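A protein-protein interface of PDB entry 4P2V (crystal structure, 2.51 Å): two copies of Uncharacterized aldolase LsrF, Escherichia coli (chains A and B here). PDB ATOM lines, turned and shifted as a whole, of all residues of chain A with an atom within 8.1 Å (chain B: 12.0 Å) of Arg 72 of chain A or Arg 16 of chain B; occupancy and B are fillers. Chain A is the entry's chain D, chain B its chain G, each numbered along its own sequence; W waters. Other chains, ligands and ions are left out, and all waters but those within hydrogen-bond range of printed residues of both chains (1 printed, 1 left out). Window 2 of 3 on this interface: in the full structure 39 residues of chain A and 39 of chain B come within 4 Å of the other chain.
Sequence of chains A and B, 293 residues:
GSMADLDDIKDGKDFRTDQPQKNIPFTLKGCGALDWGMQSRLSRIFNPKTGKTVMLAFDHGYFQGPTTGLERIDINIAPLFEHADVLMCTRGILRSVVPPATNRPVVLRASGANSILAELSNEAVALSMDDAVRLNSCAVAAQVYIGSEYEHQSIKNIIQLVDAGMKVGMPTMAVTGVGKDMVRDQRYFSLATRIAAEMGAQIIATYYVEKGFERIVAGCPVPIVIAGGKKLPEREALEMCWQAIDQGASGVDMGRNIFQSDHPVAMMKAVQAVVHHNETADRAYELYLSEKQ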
ATOM      1  N   PRO A  66     -23.684 -23.086  14.906  1.00  0.00           N
ATOM      2  CA  PRO A  66     -24.757 -23.452  13.974  1.00  0.00           C
ATOM      3  C   PRO A  66     -25.744 -22.314  13.723  1.00  0.00           C
ATOM      4  O   PRO A  66     -26.846 -22.304  14.277  1.00  0.00           O
ATOM      5  CB  PRO A  66     -25.446 -24.640  14.665  1.00  0.00           C
ATOM      6  CG  PRO A  66     -24.505 -25.081  15.744  1.00  0.00           C
ATOM      7  CD  PRO A  66     -23.744 -23.868  16.152  1.00  0.00           C
ATOM      8  N   THR A  67     -25.330 -21.369  12.881  1.00  0.00           N
ATOM      9  CA  THR A  67     -26.170 -20.249  12.489  1.00  0.00           C
ATOM     10  C   THR A  67     -27.398 -20.834  11.784  1.00  0.00           C
ATOM     11  O   THR A  67     -27.330 -21.948  11.258  1.00  0.00           O
ATOM     12  CB  THR A  67     -25.363 -19.277  11.573  1.00  0.00           C
ATOM     13  OG1 THR A  67     -24.350 -18.644  12.361  1.00  0.00           O
ATOM     14  CG2 THR A  67     -26.233 -18.173  11.003  1.00  0.00           C
ATOM     15  N   THR A  68     -28.505 -20.093  11.757  1.00  0.00           N
ATOM     16  CA  THR A  68     -29.740 -20.571  11.158  1.00  0.00           C
ATOM     17  C   THR A  68     -29.395 -20.848   9.718  1.00  0.00           C
ATOM     18  O   THR A  68     -28.834 -19.987   9.098  1.00  0.00           O
ATOM     19  CB  THR A  68     -30.858 -19.504  11.219  1.00  0.00           C
ATOM     20  OG1 THR A  68     -30.523 -18.421  10.339  1.00  0.00           O
ATOM     21  CG2 THR A  68     -31.036 -18.973  12.638  1.00  0.00           C
ATOM     22  N   GLY A  69     -29.625 -22.051   9.203  1.00  0.00           N
ATOM     23  CA  GLY A  69     -29.266 -22.364   7.820  1.00  0.00           C
ATOM     24  C   GLY A  69     -27.912 -23.036   7.584  1.00  0.00           C
ATOM     25  O   GLY A  69     -27.762 -23.722   6.570  1.00  0.00           O
ATOM     26  N   LEU A  70     -26.973 -22.904   8.532  1.00  0.00           N
ATOM     27  CA  LEU A  70     -25.657 -23.562   8.469  1.00  0.00           C
ATOM     28  C   LEU A  70     -25.655 -24.560   9.592  1.00  0.00           C
ATOM     29  O   LEU A  70     -24.591 -24.956  10.061  1.00  0.00           O
ATOM     30  CB  LEU A  70     -24.448 -22.642   8.694  1.00  0.00           C
ATOM     31  CG  LEU A  70     -23.947 -21.677   7.647  1.00  0.00           C
ATOM     32  CD1 LEU A  70     -22.607 -21.131   8.047  1.00  0.00           C
ATOM     33  CD2 LEU A  70     -23.835 -22.376   6.333  1.00  0.00           C
ATOM     34  N   GLU A  71     -26.832 -24.925  10.088  1.00  0.00           N
ATOM     35  CA  GLU A  71     -26.848 -25.962  11.104  1.00  0.00           C
ATOM     36  C   GLU A  71     -26.491 -27.285  10.391  1.00  0.00           C
ATOM     37  O   GLU A  71     -25.818 -28.164  10.949  1.00  0.00           O
ATOM     38  CB  GLU A  71     -28.195 -26.060  11.836  1.00  0.00           C
ATOM     39  CG  GLU A  71     -29.481 -25.858  11.032  1.00  0.00           C
ATOM     40  CD  GLU A  71     -29.972 -24.409  11.013  1.00  0.00           C
ATOM     41  OE1 GLU A  71     -29.686 -23.689  11.988  1.00  0.00           O
ATOM     42  OE2 GLU A  71     -30.706 -24.000  10.084  1.00  0.00           O
ATOM     43  N   ARG A  72     -26.930 -27.405   9.139  1.00  0.00           N
ATOM     44  CA  ARG A  72     -26.640 -28.592   8.336  1.00  0.00           C
ATOM     45  C   ARG A  72     -26.049 -28.230   6.969  1.00  0.00           C
ATOM     46  O   ARG A  72     -26.790 -28.102   5.992  1.00  0.00           O
ATOM     47  CB  ARG A  72     -27.918 -29.411   8.136  1.00  0.00           C
ATOM     48  CG  ARG A  72     -28.520 -29.948   9.421  1.00  0.00           C
ATOM     49  CD  ARG A  72     -27.578 -30.881  10.168  1.00  0.00           C
ATOM     50  NE  ARG A  72     -27.235 -32.087   9.419  1.00  0.00           N
ATOM     51  CZ  ARG A  72     -27.977 -33.192   9.409  1.00  0.00           C
ATOM     52  NH1 ARG A  72     -29.107 -33.239  10.103  1.00  0.00           N
ATOM     53  NH2 ARG A  72     -27.591 -34.246   8.705  1.00  0.00           N
ATOM     54  N   ILE A  73     -24.726 -28.103   6.885  1.00  0.00           N
ATOM     55  CA  ILE A  73     -24.058 -27.742   5.630  1.00  0.00           C
ATOM     56  C   ILE A  73     -24.223 -28.740   4.486  1.00  0.00           C
ATOM     57  O   ILE A  73     -24.410 -28.355   3.331  1.00  0.00           O
ATOM     58  CB  ILE A  73     -22.543 -27.586   5.859  1.00  0.00           C
ATOM     59  CG1 ILE A  73     -22.263 -26.574   6.954  1.00  0.00           C
ATOM     60  CG2 ILE A  73     -21.870 -27.108   4.580  1.00  0.00           C
ATOM     61  CD1 ILE A  73     -22.454 -25.247   6.462  1.00  0.00           C
ATOM     62  N   ASP A  74     -24.170 -30.022   4.824  1.00  0.00           N
ATOM     63  CA  ASP A  74     -24.247 -31.089   3.830  1.00  0.00           C
ATOM     64  C   ASP A  74     -25.581 -31.234   3.115  1.00  0.00           C
ATOM     65  O   ASP A  74     -25.628 -31.797   2.041  1.00  0.00           O
ATOM     66  CB  ASP A  74     -23.964 -32.407   4.494  1.00  0.00           C
ATOM     67  CG  ASP A  74     -25.059 -32.791   5.488  1.00  0.00           C
ATOM     68  OD1 ASP A  74     -25.485 -31.936   6.285  1.00  0.00           O
ATOM     69  OD2 ASP A  74     -25.472 -33.964   5.471  1.00  0.00           O
ATOM     70  N   ILE A  75     -26.664 -30.730   3.692  1.00  0.00           N
ATOM     71  CA  ILE A  75     -27.982 -30.984   3.121  1.00  0.00           C
ATOM     72  C   ILE A  75     -28.518 -29.717   2.479  1.00  0.00           C
ATOM     73  O   ILE A  75     -29.080 -29.762   1.387  1.00  0.00           O
ATOM     74  CB  ILE A  75     -28.979 -31.531   4.182  1.00  0.00           C
ATOM     75  CG1 ILE A  75     -28.405 -32.791   4.863  1.00  0.00           C
ATOM     76  CG2 ILE A  75     -30.407 -31.642   3.598  1.00  0.00           C
ATOM     77  CD1 ILE A  75     -29.282 -33.363   5.933  1.00  0.00           C
ATOM     78  N   ASN A  76     -28.332 -28.582   3.143  1.00  0.00           N
ATOM     79  CA  ASN A  76     -28.893 -27.331   2.649  1.00  0.00           C
ATOM     80  C   ASN A  76     -27.877 -26.415   1.960  1.00  0.00           C
ATOM     81  O   ASN A  76     -28.265 -25.468   1.272  1.00  0.00           O
ATOM     82  CB  ASN A  76     -29.565 -26.565   3.797  1.00  0.00           C
ATOM     83  CG  ASN A  76     -30.603 -27.399   4.527  1.00  0.00           C
ATOM     84  OD1 ASN A  76     -31.392 -28.107   3.901  1.00  0.00           O
ATOM     85  ND2 ASN A  76     -30.627 -27.296   5.851  1.00  0.00           N
ATOM     86  N   ILE A  77     -26.585 -26.696   2.105  1.00  0.00           N
ATOM     87  CA  ILE A  77     -25.585 -25.864   1.437  1.00  0.00           C
ATOM     88  C   ILE A  77     -24.877 -26.630   0.324  1.00  0.00           C
ATOM     89  O   ILE A  77     -24.398 -26.040  -0.649  1.00  0.00           O
ATOM     90  CB  ILE A  77     -24.525 -25.338   2.433  1.00  0.00           C
ATOM     91  CG1 ILE A  77     -25.188 -24.872   3.726  1.00  0.00           C
ATOM     92  CG2 ILE A  77     -23.683 -24.230   1.807  1.00  0.00           C
ATOM     93  CD1 ILE A  77     -26.201 -23.779   3.534  1.00  0.00           C
ATOM     94  N   ALA A  78     -24.814 -27.948   0.473  1.00  0.00           N
ATOM     95  CA  ALA A  78     -24.214 -28.804  -0.545  1.00  0.00           C
ATOM     96  C   ALA A  78     -24.868 -28.671  -1.928  1.00  0.00           C
ATOM     97  O   ALA A  78     -24.157 -28.615  -2.928  1.00  0.00           O
ATOM     98  CB  ALA A  78     -24.229 -30.255  -0.092  1.00  0.00           C
ATOM     99  N   PRO A  79     -26.215 -28.629  -2.004  1.00  0.00           N
ATOM    100  CA  PRO A  79     -26.763 -28.482  -3.362  1.00  0.00           C
ATOM    101  C   PRO A  79     -26.547 -27.103  -3.993  1.00  0.00           C
ATOM    102  O   PRO A  79     -26.949 -26.897  -5.140  1.00  0.00           O
ATOM    103  CB  PRO A  79     -28.266 -28.737  -3.184  1.00  0.00           C
ATOM    104  CG  PRO A  79     -28.462 -29.245  -1.816  1.00  0.00           C
ATOM    105  CD  PRO A  79     -27.246 -28.980  -1.007  1.00  0.00           C
ATOM    106  N   ILE A  93     -14.913 -27.390   7.752  1.00  0.00           N
ATOM    107  CA  ILE A  93     -16.118 -27.572   6.955  1.00  0.00           C
ATOM    108  C   ILE A  93     -15.731 -28.128   5.593  1.00  0.00           C
ATOM    109  O   ILE A  93     -16.410 -28.997   5.047  1.00  0.00           O
ATOM    110  CB  ILE A  93     -16.894 -26.244   6.779  1.00  0.00           C
ATOM    111  CG1 ILE A  93     -17.567 -25.842   8.091  1.00  0.00           C
ATOM    112  CG2 ILE A  93     -17.940 -26.359   5.680  1.00  0.00           C
ATOM    113  CD1 ILE A  93     -18.528 -26.877   8.628  1.00  0.00           C
ATOM    114  N   VAL A  97     -17.509 -31.802   5.022  1.00  0.00           N
ATOM    115  CA  VAL A  97     -18.797 -31.877   4.335  1.00  0.00           C
ATOM    116  C   VAL A  97     -18.772 -31.338   2.907  1.00  0.00           C
ATOM    117  O   VAL A  97     -19.753 -31.469   2.178  1.00  0.00           O
ATOM    118  CB  VAL A  97     -19.879 -31.090   5.099  1.00  0.00           C
ATOM    119  CG1 VAL A  97     -20.067 -31.664   6.488  1.00  0.00           C
ATOM    120  CG2 VAL A  97     -19.487 -29.637   5.210  1.00  0.00           C
ATOM    121  N   PHE A 259     -28.107 -18.708   1.956  1.00  0.00           N
ATOM    122  CA  PHE A 259     -28.478 -19.959   2.614  1.00  0.00           C
ATOM    123  C   PHE A 259     -29.736 -19.852   3.475  1.00  0.00           C
ATOM    124  O   PHE A 259     -30.368 -20.863   3.781  1.00  0.00           O
ATOM    125  CB  PHE A 259     -27.304 -20.564   3.394  1.00  0.00           C
ATOM    126  CG  PHE A 259     -26.657 -19.622   4.367  1.00  0.00           C
ATOM    127  CD1 PHE A 259     -27.353 -19.150   5.466  1.00  0.00           C
ATOM    128  CD2 PHE A 259     -25.340 -19.231   4.195  1.00  0.00           C
ATOM    129  CE1 PHE A 259     -26.752 -18.293   6.367  1.00  0.00           C
ATOM    130  CE2 PHE A 259     -24.732 -18.375   5.092  1.00  0.00           C
ATOM    131  CZ  PHE A 259     -25.439 -17.906   6.181  1.00  0.00           C
ATOM    132  N   ASP B  11     -35.532 -23.086  18.136  1.00  0.00           N
ATOM    133  CA  ASP B  11     -35.279 -21.775  17.550  1.00  0.00           C
ATOM    134  C   ASP B  11     -35.932 -21.677  16.157  1.00  0.00           C
ATOM    135  O   ASP B  11     -37.081 -22.067  15.959  1.00  0.00           O
ATOM    136  CB  ASP B  11     -33.764 -21.527  17.456  1.00  0.00           C
ATOM    137  CG  ASP B  11     -33.425 -20.090  17.083  1.00  0.00           C
ATOM    138  OD1 ASP B  11     -34.361 -19.258  17.051  1.00  0.00           O
ATOM    139  OD2 ASP B  11     -32.239 -19.786  16.846  1.00  0.00           O
ATOM    140  N   GLY B  12     -35.192 -21.060  15.241  1.00  0.00           N
ATOM    141  CA  GLY B  12     -35.452 -20.988  13.819  1.00  0.00           C
ATOM    142  C   GLY B  12     -34.507 -21.999  13.194  1.00  0.00           C
ATOM    143  O   GLY B  12     -34.183 -21.929  12.003  1.00  0.00           O
ATOM    144  N   LYS B  13     -33.989 -22.883  14.047  1.00  0.00           N
ATOM    145  CA  LYS B  13     -33.036 -23.915  13.652  1.00  0.00           C
ATOM    146  C   LYS B  13     -33.686 -25.154  13.068  1.00  0.00           C
ATOM    147  O   LYS B  13     -34.763 -25.566  13.496  1.00  0.00           O
ATOM    148  CB  LYS B  13     -32.203 -24.369  14.853  1.00  0.00           C
ATOM    149  CG  LYS B  13     -30.911 -23.630  15.171  1.00  0.00           C
ATOM    150  CD  LYS B  13     -30.931 -22.126  15.073  1.00  0.00           C
ATOM    151  CE  LYS B  13     -29.740 -21.592  15.871  1.00  0.00           C
ATOM    152  NZ  LYS B  13     -29.721 -20.118  16.031  1.00  0.00           N
ATOM    153  N   ASP B  14     -33.027 -25.746  12.080  1.00  0.00           N
ATOM    154  CA  ASP B  14     -33.492 -27.006  11.524  1.00  0.00           C
ATOM    155  C   ASP B  14     -32.299 -27.952  11.404  1.00  0.00           C
ATOM    156  O   ASP B  14     -31.559 -27.884  10.426  1.00  0.00           O
ATOM    157  CB  ASP B  14     -34.169 -26.790  10.169  1.00  0.00           C
ATOM    158  CG  ASP B  14     -34.770 -28.063   9.612  1.00  0.00           C
ATOM    159  OD1 ASP B  14     -34.761 -29.087  10.327  1.00  0.00           O
ATOM    160  OD2 ASP B  14     -35.273 -28.039   8.469  1.00  0.00           O
ATOM    161  N   PHE B  15     -32.123 -28.851  12.372  1.00  0.00           N
ATOM    162  CA  PHE B  15     -30.959 -29.746  12.363  1.00  0.00           C
ATOM    163  C   PHE B  15     -31.217 -31.068  11.654  1.00  0.00           C
ATOM    164  O   PHE B  15     -30.295 -31.865  11.482  1.00  0.00           O
ATOM    165  CB  PHE B  15     -30.497 -30.061  13.785  1.00  0.00           C
ATOM    166  CG  PHE B  15     -29.949 -28.883  14.525  1.00  0.00           C
ATOM    167  CD1 PHE B  15     -30.800 -27.972  15.114  1.00  0.00           C
ATOM    168  CD2 PHE B  15     -28.585 -28.677  14.622  1.00  0.00           C
ATOM    169  CE1 PHE B  15     -30.305 -26.899  15.808  1.00  0.00           C
ATOM    170  CE2 PHE B  15     -28.083 -27.586  15.310  1.00  0.00           C
ATOM    171  CZ  PHE B  15     -28.950 -26.697  15.904  1.00  0.00           C
ATOM    172  N   ARG B  16     -32.459 -31.287  11.237  1.00  0.00           N
ATOM    173  CA  ARG B  16     -32.849 -32.530  10.576  1.00  0.00           C
ATOM    174  C   ARG B  16     -32.298 -33.767  11.295  1.00  0.00           C
ATOM    175  O   ARG B  16     -31.576 -34.561  10.692  1.00  0.00           O
ATOM    176  CB  ARG B  16     -32.354 -32.511   9.129  1.00  0.00           C
ATOM    177  CG  ARG B  16     -33.033 -31.463   8.272  1.00  0.00           C
ATOM    178  CD  ARG B  16     -32.535 -31.509   6.840  1.00  0.00           C
ATOM    179  NE  ARG B  16     -33.174 -30.488   6.017  1.00  0.00           N
ATOM    180  CZ  ARG B  16     -34.366 -30.627   5.448  1.00  0.00           C
ATOM    181  NH1 ARG B  16     -35.051 -31.749   5.613  1.00  0.00           N
ATOM    182  NH2 ARG B  16     -34.873 -29.646   4.713  1.00  0.00           N
ATOM    183  N   THR B  17     -32.626 -33.924  12.576  1.00  0.00           N
ATOM    184  CA  THR B  17     -32.124 -35.060  13.356  1.00  0.00           C
ATOM    185  C   THR B  17     -32.487 -36.427  12.790  1.00  0.00           C
ATOM    186  O   THR B  17     -31.783 -37.410  13.019  1.00  0.00           O
ATOM    187  CB  THR B  17     -32.630 -35.010  14.812  1.00  0.00           C
ATOM    188  OG1 THR B  17     -32.160 -36.168  15.512  1.00  0.00           O
ATOM    189  CG2 THR B  17     -34.146 -34.969  14.866  1.00  0.00           C
ATOM    190  N   ASP B  18     -33.588 -36.490  12.056  1.00  0.00           N
ATOM    191  CA  ASP B  18     -33.975 -37.717  11.374  1.00  0.00           C
ATOM    192  C   ASP B  18     -33.019 -38.093  10.245  1.00  0.00           C
ATOM    193  O   ASP B  18     -32.947 -39.253   9.843  1.00  0.00           O
ATOM    194  CB  ASP B  18     -35.407 -37.593  10.850  1.00  0.00           C
ATOM    195  CG  ASP B  18     -35.575 -36.449   9.870  1.00  0.00           C
ATOM    196  OD1 ASP B  18     -35.045 -35.349  10.137  1.00  0.00           O
ATOM    197  OD2 ASP B  18     -36.252 -36.643   8.838  1.00  0.00           O
ATOM    198  N   GLN B  19     -32.284 -37.118   9.730  1.00  0.00           N
ATOM    199  CA  GLN B  19     -31.480 -37.363   8.539  1.00  0.00           C
ATOM    200  C   GLN B  19     -29.968 -37.310   8.800  1.00  0.00           C
ATOM    201  O   GLN B  19     -29.384 -36.229   8.891  1.00  0.00           O
ATOM    202  CB  GLN B  19     -31.871 -36.369   7.455  1.00  0.00           C
ATOM    203  CG  GLN B  19     -31.403 -36.771   6.071  1.00  0.00           C
ATOM    204  CD  GLN B  19     -31.889 -35.823   4.998  1.00  0.00           C
ATOM    205  OE1 GLN B  19     -32.856 -35.083   5.191  1.00  0.00           O
ATOM    206  NE2 GLN B  19     -31.202 -35.823   3.867  1.00  0.00           N
ATOM    207  N   PRO B  20     -29.341 -38.488   8.946  1.00  0.00           N
ATOM    208  CA  PRO B  20     -27.903 -38.597   9.194  1.00  0.00           C
ATOM    209  C   PRO B  20     -27.053 -38.046   8.047  1.00  0.00           C
ATOM    210  O   PRO B  20     -27.443 -38.103   6.881  1.00  0.00           O
ATOM    211  CB  PRO B  20     -27.680 -40.105   9.381  1.00  0.00           C
ATOM    212  CG  PRO B  20     -28.843 -40.770   8.769  1.00  0.00           C
ATOM    213  CD  PRO B  20     -29.944 -39.777   8.572  1.00  0.00           C
ATOM    214  N   GLN B  21     -25.893 -37.508   8.412  1.00  0.00           N
ATOM    215  CA  GLN B  21     -24.882 -37.055   7.467  1.00  0.00           C
ATOM    216  C   GLN B  21     -24.219 -38.229   6.749  1.00  0.00           C
ATOM    217  O   GLN B  21     -23.940 -39.258   7.361  1.00  0.00           O
ATOM    218  CB  GLN B  21     -23.798 -36.256   8.196  1.00  0.00           C
ATOM    219  CG  GLN B  21     -23.433 -34.883   7.640  1.00  0.00           C
ATOM    220  CD  GLN B  21     -22.738 -34.985   6.280  1.00  0.00           C
ATOM    221  OE1 GLN B  21     -23.187 -35.714   5.404  1.00  0.00           O
ATOM    222  NE2 GLN B  21     -21.593 -34.349   6.142  1.00  0.00           N
ATOM    223  N   LYS B  22     -23.954 -38.082   5.455  1.00  0.00           N
ATOM    224  CA  LYS B  22     -23.343 -39.187   4.738  1.00  0.00           C
ATOM    225  C   LYS B  22     -22.181 -38.660   3.910  1.00  0.00           C
ATOM    226  O   LYS B  22     -22.304 -37.650   3.215  1.00  0.00           O
ATOM    227  CB  LYS B  22     -24.363 -39.903   3.857  1.00  0.00           C
ATOM    228  CG  LYS B  22     -24.150 -41.406   3.881  1.00  0.00           C
ATOM    229  CD  LYS B  22     -25.214 -42.182   3.143  1.00  0.00           C
ATOM    230  CE  LYS B  22     -25.122 -43.657   3.516  1.00  0.00           C
ATOM    231  NZ  LYS B  22     -23.795 -44.263   3.264  1.00  0.00           N
ATOM    232  N   ASN B  23     -21.048 -39.344   3.999  1.00  0.00           N
ATOM    233  CA  ASN B  23     -19.861 -38.949   3.260  1.00  0.00           C
ATOM    234  C   ASN B  23     -20.077 -39.200   1.777  1.00  0.00           C
ATOM    235  O   ASN B  23     -20.631 -40.228   1.394  1.00  0.00           O
ATOM    236  CB  ASN B  23     -18.633 -39.708   3.760  1.00  0.00           C
ATOM    237  CG  ASN B  23     -18.214 -39.285   5.152  1.00  0.00           C
ATOM    238  OD1 ASN B  23     -18.767 -38.348   5.725  1.00  0.00           O
ATOM    239  ND2 ASN B  23     -17.239 -39.990   5.713  1.00  0.00           N
ATOM    240  N   ILE B  24     -19.665 -38.245   0.949  1.00  0.00           N
ATOM    241  CA  ILE B  24     -19.787 -38.408  -0.492  1.00  0.00           C
ATOM    242  C   ILE B  24     -18.538 -39.112  -1.019  1.00  0.00           C
ATOM    243  O   ILE B  24     -17.449 -38.530  -0.985  1.00  0.00           O
ATOM    244  CB  ILE B  24     -19.950 -37.038  -1.208  1.00  0.00           C
ATOM    245  CG1 ILE B  24     -21.149 -36.264  -0.660  1.00  0.00           C
ATOM    246  CG2 ILE B  24     -19.986 -37.209  -2.733  1.00  0.00           C
ATOM    247  CD1 ILE B  24     -22.459 -37.002  -0.749  1.00  0.00           C
HETATM  248  O   HOH W   1     -21.567 -33.697   2.709  1.00  0.00           O
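NH1 of Arg 72 of chain A is in hydrogen-bond range of O of Arg 16 of chain B (2.9 Å). The backbone carbonyl oxygen (O) of Gln 19 of chain B is in hydrogen-bond range of the guanidinium group (NH2) of Arg 72 of chain A, at 2.7 Å. OD2 of Asp 74 of chain A lies close to OE1 of Gln 21 of chain B (2.9 Å). The backbone carbonyl oxygen (O) of Phe 15 of chain B lies close to the guanidinium group (NH1) of Arg 72 of chain A, 2.3 Å away.
The side-chain carboxylate of Glu 71 of chain A lies close to the backbone NH of Gly 69 of chain A, at 3.2 Å. The guanidinium group of Arg 72 of chain A is in salt-bridge range of the side-chain carboxylate of Asp 74 of chain A, at 3.6 Å. NZ of Lys 13 of chain B lies within salt-bridge range of OD2 of Asp 11 of chain B, at 2.7 Å. OD1 of Asp 14 of chain B sits at hydrogen-bond distance from N of Arg 16 of chain B, 3.3 Å away.
Among the printed residues, pairs that only touch across the chains: Glu 71 of chain A with Asp 14 of chain B (3.0 Å), Val 97 of chain A with Gln 21 of chain B (3.1 Å), Pro 66 of chain A with Lys 13 of chain B (3.4 Å), Glu 71 of chain A with Lys 13 of chain B (3.4 Å), Asn 76 of chain A with Arg 16 of chain B (3.6 Å), Arg 72 of chain A with Gln 21 of chain B (3.7 Å), Ile 75 of chain A with Gln 19 of chain B (3.7 Å), Glu 71 of chain A with Phe 15 of chain B (3.8 Å), Arg 72 of chain A with Asp 14 of chain B (3.8 Å), Thr 68 of chain A with Lys 13 of chain B (3.8 Å), Ile 75 of chain A with Arg 16 of chain B (3.9 Å) and Arg 72 of chain A with Pro 20 of chain B (3.9 Å).
Of the printed residues of chain B, Pro 66 of chain A touches Lys 13 (3.4 Å). No residue of chain B comes within 4 Å of Gly 69 of chain A. Leu 70 of chain A touches none of the printed residues of chain B. Glu 71 of chain A touches three residues of chain B. Arg 72 of chain A touches just these residues of chain B: Asp 14 (3.8 Å), Phe 15 (2.3 Å), Arg 16 (2.9 Å), Gln 19 (2.7 Å), Pro 20 (3.9 Å) and Gln 21 (3.7 Å). No residue of chain B comes within 4 Å of Ile 73 of chain A. Ile 77 of chain A touches none of the printed residues of chain B. Arg 16 of chain B touches just these residues of chain A: Arg 72 (2.9 Å), Ile 75 (3.9 Å) and Asn 76 (3.6 Å). Of the printed residues of chain A, Pro 20 of chain B touches Arg 72 (3.9 Å). The nearest printed residue of chain B that does not touch Thr 68 of chain A is Gly 12 of chain B (4.2 Å).
Of the 17 printed residues of chain A, 8 touch a printed residue of chain B. Hydrophobic or aromatic side chains of chain A that line the printed part of chain B: Ile 75 and Val 97.
No position is printed for both chains.
Water W1 bridges O of Val 97 of chain A and NE2 of Gln 21 of chain B.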
